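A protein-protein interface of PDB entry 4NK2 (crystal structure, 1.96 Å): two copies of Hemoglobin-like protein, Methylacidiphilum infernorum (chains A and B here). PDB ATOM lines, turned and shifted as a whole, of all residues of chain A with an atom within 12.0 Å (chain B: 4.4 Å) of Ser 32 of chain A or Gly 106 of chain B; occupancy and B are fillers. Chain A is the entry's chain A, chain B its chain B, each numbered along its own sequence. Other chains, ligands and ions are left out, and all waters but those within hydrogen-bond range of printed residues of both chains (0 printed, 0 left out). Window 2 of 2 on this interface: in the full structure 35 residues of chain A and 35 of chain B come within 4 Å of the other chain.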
ATOM      1  N   ALA A  30      24.145  -4.521 -17.661  1.00  0.00           N
ATOM      2  CA  ALA A  30      24.163  -5.879 -17.116  1.00  0.00           C
ATOM      3  C   ALA A  30      25.207  -6.039 -16.013  1.00  0.00           C
ATOM      4  O   ALA A  30      26.406  -6.141 -16.293  1.00  0.00           O
ATOM      5  CB  ALA A  30      24.409  -6.893 -18.228  1.00  0.00           C
ATOM      6  N   GLU A  31      24.750  -6.058 -14.763  1.00  0.00           N
ATOM      7  CA  GLU A  31      25.638  -6.284 -13.623  1.00  0.00           C
ATOM      8  C   GLU A  31      24.892  -6.946 -12.463  1.00  0.00           C
ATOM      9  O   GLU A  31      23.689  -7.195 -12.540  1.00  0.00           O
ATOM     10  CB  GLU A  31      26.289  -4.972 -13.166  1.00  0.00           C
ATOM     11  CG  GLU A  31      25.375  -4.072 -12.340  1.00  0.00           C
ATOM     12  CD  GLU A  31      25.603  -2.594 -12.609  1.00  0.00           C
ATOM     13  OE1 GLU A  31      26.395  -2.263 -13.519  1.00  0.00           O
ATOM     14  OE2 GLU A  31      24.983  -1.763 -11.913  1.00  0.00           O
ATOM     15  N   SER A  32      25.615  -7.232 -11.388  1.00  0.00           N
ATOM     16  CA  SER A  32      25.013  -7.846 -10.211  1.00  0.00           C
ATOM     17  C   SER A  32      23.689  -7.171  -9.835  1.00  0.00           C
ATOM     18  O   SER A  32      23.639  -5.962  -9.583  1.00  0.00           O
ATOM     19  CB  SER A  32      25.985  -7.803  -9.032  1.00  0.00           C
ATOM     20  OG  SER A  32      25.440  -8.472  -7.913  1.00  0.00           O
ATOM     21  N   GLY A  33      22.623  -7.959  -9.823  1.00  0.00           N
ATOM     22  CA  GLY A  33      21.301  -7.470  -9.502  1.00  0.00           C
ATOM     23  C   GLY A  33      20.525  -7.073 -10.732  1.00  0.00           C
ATOM     24  O   GLY A  33      19.314  -6.979 -10.697  1.00  0.00           O
ATOM     25  N   SER A  34      21.233  -6.842 -11.825  1.00  0.00           N
ATOM     26  CA  SER A  34      20.596  -6.427 -13.079  1.00  0.00           C
ATOM     27  C   SER A  34      19.493  -7.400 -13.503  1.00  0.00           C
ATOM     28  O   SER A  34      19.545  -8.592 -13.188  1.00  0.00           O
ATOM     29  CB  SER A  34      21.634  -6.323 -14.204  1.00  0.00           C
ATOM     30  OG  SER A  34      22.681  -5.424 -13.878  1.00  0.00           O
ATOM     31  N   ILE A  35      18.497  -6.883 -14.215  1.00  0.00           N
ATOM     32  CA  ILE A  35      17.480  -7.717 -14.845  1.00  0.00           C
ATOM     33  C   ILE A  35      17.396  -7.378 -16.327  1.00  0.00           C
ATOM     34  O   ILE A  35      16.781  -6.376 -16.688  1.00  0.00           O
ATOM     35  CB  ILE A  35      16.086  -7.490 -14.222  1.00  0.00           C
ATOM     36  CG1 ILE A  35      16.067  -7.946 -12.763  1.00  0.00           C
ATOM     37  CG2 ILE A  35      15.016  -8.227 -15.019  1.00  0.00           C
ATOM     38  CD1 ILE A  35      14.734  -7.730 -12.073  1.00  0.00           C
ATOM     39  N   CYS A  36      18.016  -8.189 -17.183  1.00  0.00           N
ATOM     40  CA  CYS A  36      17.875  -8.004 -18.626  1.00  0.00           C
ATOM     41  C   CYS A  36      16.504  -8.509 -19.047  1.00  0.00           C
ATOM     42  O   CYS A  36      16.232  -9.704 -18.949  1.00  0.00           O
ATOM     43  CB  CYS A  36      18.944  -8.791 -19.374  1.00  0.00           C
ATOM     44  SG  CYS A  36      20.616  -8.406 -18.867  1.00  0.00           S
ATOM     45  N   PRO B  50      22.624 -12.369 -10.522  1.00  0.00           N
ATOM     46  CA  PRO B  50      22.632 -12.688  -9.086  1.00  0.00           C
ATOM     47  C   PRO B  50      22.764 -11.415  -8.240  1.00  0.00           C
ATOM     48  O   PRO B  50      23.437 -10.475  -8.668  1.00  0.00           O
ATOM     49  CB  PRO B  50      23.883 -13.562  -8.925  1.00  0.00           C
ATOM     50  CG  PRO B  50      24.229 -14.037 -10.329  1.00  0.00           C
ATOM     51  CD  PRO B  50      23.790 -12.920 -11.234  1.00  0.00           C
ATOM     52  N   SER B  51      22.124 -11.366  -7.074  1.00  0.00           N
ATOM     53  CA  SER B  51      22.359 -10.254  -6.150  1.00  0.00           C
ATOM     54  C   SER B  51      23.698 -10.441  -5.448  1.00  0.00           C
ATOM     55  O   SER B  51      24.259 -11.551  -5.450  1.00  0.00           O
ATOM     56  CB  SER B  51      21.254 -10.169  -5.106  1.00  0.00           C
ATOM     57  OG  SER B  51      21.481 -11.092  -4.059  1.00  0.00           O
ATOM     58  N   LYS B  52      24.212  -9.377  -4.849  1.00  0.00           N
ATOM     59  CA  LYS B  52      25.497  -9.430  -4.168  1.00  0.00           C
ATOM     60  C   LYS B  52      25.535 -10.437  -3.023  1.00  0.00           C
ATOM     61  O   LYS B  52      26.592 -10.792  -2.572  1.00  0.00           O
ATOM     62  CB  LYS B  52      25.903  -8.053  -3.661  1.00  0.00           C
ATOM     63  CG  LYS B  52      24.974  -7.511  -2.596  1.00  0.00           C
ATOM     64  CD  LYS B  52      25.522  -6.267  -1.924  1.00  0.00           C
ATOM     65  CE  LYS B  52      24.807  -5.993  -0.610  1.00  0.00           C
ATOM     66  NZ  LYS B  52      23.425  -6.557  -0.580  1.00  0.00           N
ATOM     67  N   TYR B  55      27.968 -13.443  -3.884  1.00  0.00           N
ATOM     68  CA  TYR B  55      29.389 -13.236  -3.633  1.00  0.00           C
ATOM     69  C   TYR B  55      29.678 -13.327  -2.133  1.00  0.00           C
ATOM     70  O   TYR B  55      30.687 -13.899  -1.719  1.00  0.00           O
ATOM     71  CB  TYR B  55      29.845 -11.881  -4.177  1.00  0.00           C
ATOM     72  CG  TYR B  55      31.268 -11.507  -3.790  1.00  0.00           C
ATOM     73  CD1 TYR B  55      32.353 -12.205  -4.294  1.00  0.00           C
ATOM     74  CD2 TYR B  55      31.518 -10.437  -2.943  1.00  0.00           C
ATOM     75  CE1 TYR B  55      33.648 -11.860  -3.956  1.00  0.00           C
ATOM     76  CE2 TYR B  55      32.806 -10.080  -2.601  1.00  0.00           C
ATOM     77  CZ  TYR B  55      33.869 -10.797  -3.107  1.00  0.00           C
ATOM     78  OH  TYR B  55      35.162 -10.452  -2.772  1.00  0.00           O
ATOM     79  N   VAL B 102      32.770 -14.014 -10.675  1.00  0.00           N
ATOM     80  CA  VAL B 102      33.036 -13.278  -9.437  1.00  0.00           C
ATOM     81  C   VAL B 102      32.420 -11.878  -9.497  1.00  0.00           C
ATOM     82  O   VAL B 102      31.692 -11.466  -8.588  1.00  0.00           O
ATOM     83  CB  VAL B 102      34.548 -13.189  -9.136  1.00  0.00           C
ATOM     84  CG1 VAL B 102      34.813 -12.213  -8.004  1.00  0.00           C
ATOM     85  CG2 VAL B 102      35.104 -14.565  -8.780  1.00  0.00           C
ATOM     86  N   GLU B 103      32.680 -11.149 -10.575  1.00  0.00           N
ATOM     87  CA  GLU B 103      32.115  -9.803 -10.696  1.00  0.00           C
ATOM     88  C   GLU B 103      30.586  -9.811 -10.732  1.00  0.00           C
ATOM     89  O   GLU B 103      29.936  -9.017 -10.046  1.00  0.00           O
ATOM     90  CB  GLU B 103      32.678  -9.068 -11.925  1.00  0.00           C
ATOM     91  CG  GLU B 103      31.951  -7.750 -12.234  1.00  0.00           C
ATOM     92  CD  GLU B 103      32.656  -6.903 -13.295  1.00  0.00           C
ATOM     93  OE1 GLU B 103      33.800  -7.241 -13.681  1.00  0.00           O
ATOM     94  OE2 GLU B 103      32.059  -5.896 -13.737  1.00  0.00           O
ATOM     95  N   MET B 104      30.002 -10.703 -11.527  1.00  0.00           N
ATOM     96  CA  MET B 104      28.552 -10.677 -11.721  1.00  0.00           C
ATOM     97  C   MET B 104      27.777 -11.147 -10.484  1.00  0.00           C
ATOM     98  O   MET B 104      26.608 -10.803 -10.306  1.00  0.00           O
ATOM     99  CB  MET B 104      28.167 -11.487 -12.962  1.00  0.00           C
ATOM    100  CG  MET B 104      28.693 -10.886 -14.262  1.00  0.00           C
ATOM    101  SD  MET B 104      28.075  -9.205 -14.473  1.00  0.00           S
ATOM    102  CE  MET B 104      29.519  -8.396 -15.162  1.00  0.00           C
ATOM    103  N   CYS B 105      28.432 -11.925  -9.625  1.00  0.00           N
ATOM    104  CA  CYS B 105      27.831 -12.311  -8.352  1.00  0.00           C
ATOM    105  C   CYS B 105      27.993 -11.215  -7.298  1.00  0.00           C
ATOM    106  O   CYS B 105      27.518 -11.355  -6.165  1.00  0.00           O
ATOM    107  CB  CYS B 105      28.435 -13.627  -7.859  1.00  0.00           C
ATOM    108  SG  CYS B 105      27.930 -15.028  -8.875  1.00  0.00           S
ATOM    109  N   GLY B 106      28.654 -10.119  -7.678  1.00  0.00           N
ATOM    110  CA  GLY B 106      28.759  -8.960  -6.806  1.00  0.00           C
ATOM    111  C   GLY B 106      30.133  -8.766  -6.193  1.00  0.00           C
ATOM    112  O   GLY B 106      30.281  -8.024  -5.223  1.00  0.00           O
ATOM    113  N   GLY B 107      31.142  -9.425  -6.749  1.00  0.00           N
ATOM    114  CA  GLY B 107      32.503  -9.227  -6.286  1.00  0.00           C
ATOM    115  C   GLY B 107      33.146  -8.041  -6.984  1.00  0.00           C
ATOM    116  O   GLY B 107      32.450  -7.246  -7.614  1.00  0.00           O
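Met 104 of chain B touches Ala 30 of chain A (SD to O, 3.9 Å). Glu 31 of chain A touches Met 104 of chain B (CA to SD, 3.9 Å). Ser 32 of chain A touches Ser 51 of chain B. Ser 32 of chain A touches Met 104 of chain B. C of Cys 105 of chain B touches OG of Ser 32 of chain A, at 3.8 Å. Gly 106 of chain B touches Ser 32 of chain A (CA to OG, 3.5 Å).
O of Glu 31 of chain A is in hydrogen-bond range of OG of Ser 34 of chain A (2.4 Å). O of Cys 105 of chain B sits close to N of Tyr 55 of chain B.
No position is printed for both chains. Of the 9 pairs that touch across the chains among the printed residues, none has its exchanged pair printed and touching as well.
Printed residues of chain B within 4 Å of Ala 30 of chain A: Met 104. Of the printed residues of chain B, Glu 31 of chain A touches Met 104 (3.9 Å). Of the printed residues of chain B, Ser 32 of chain A touches Pro 50 (2.9 Å), Ser 51 (3.6 Å), Lys 52 (3.4 Å), Met 104 (3.3 Å), Cys 105 (3.8 Å) and Gly 106 (3.5 Å). Of the printed residues of chain B, Gly 33 of chain A touches Pro 50. Ser 51 of chain B touches just one residue of chain A: Ser 32. Of chain A, only Ser 32 comes within 4 Å of Lys 52 of chain B. No residue of chain A comes within 4 Å of Tyr 55 of chain B. No residue of chain A comes within 4 Å of Val 102 of chain B. Glu 103 of chain B touches none of the printed residues of chain A. Of the printed residues of chain A, Gly 106 of chain B touches Ser 32 (3.5 Å). The nearest residue of chain A that does not touch Gly 106 of chain B is Gly 33 of chain A (6.8 Å).
Of the 7 printed residues of chain A, 4 touch a printed residue of chain B. Printed residues of chain A that touch a printed residue of chain B: Ala 30, Glu 31, Ser 32 and Gly 33. Along chain A the printed residues that touch a printed residue of chain B span positions 30 to 33. Hydrophobic or aromatic side chains of chain B that line the printed part of chain A: Met 104. Among the printed residues, 9 pairs touch across the chains. Among the printed residues, no Asp or Glu carboxylate lies within 4 Å of a Lys or Arg side-chain nitrogen of the other chain.
N of Gly 33 of chain A sits at hydrogen-bond distance from O of Pro 50 of chain B (2.9 Å). O of Pro 50 of chain B sits at hydrogen-bond distance from OG of Ser 32 of chain A (2.9 Å). The side-chain hydroxyl of Ser 32 of chain A is in hydrogen-bond range of the backbone NH of Lys 52 of chain B, 3.4 Å away.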
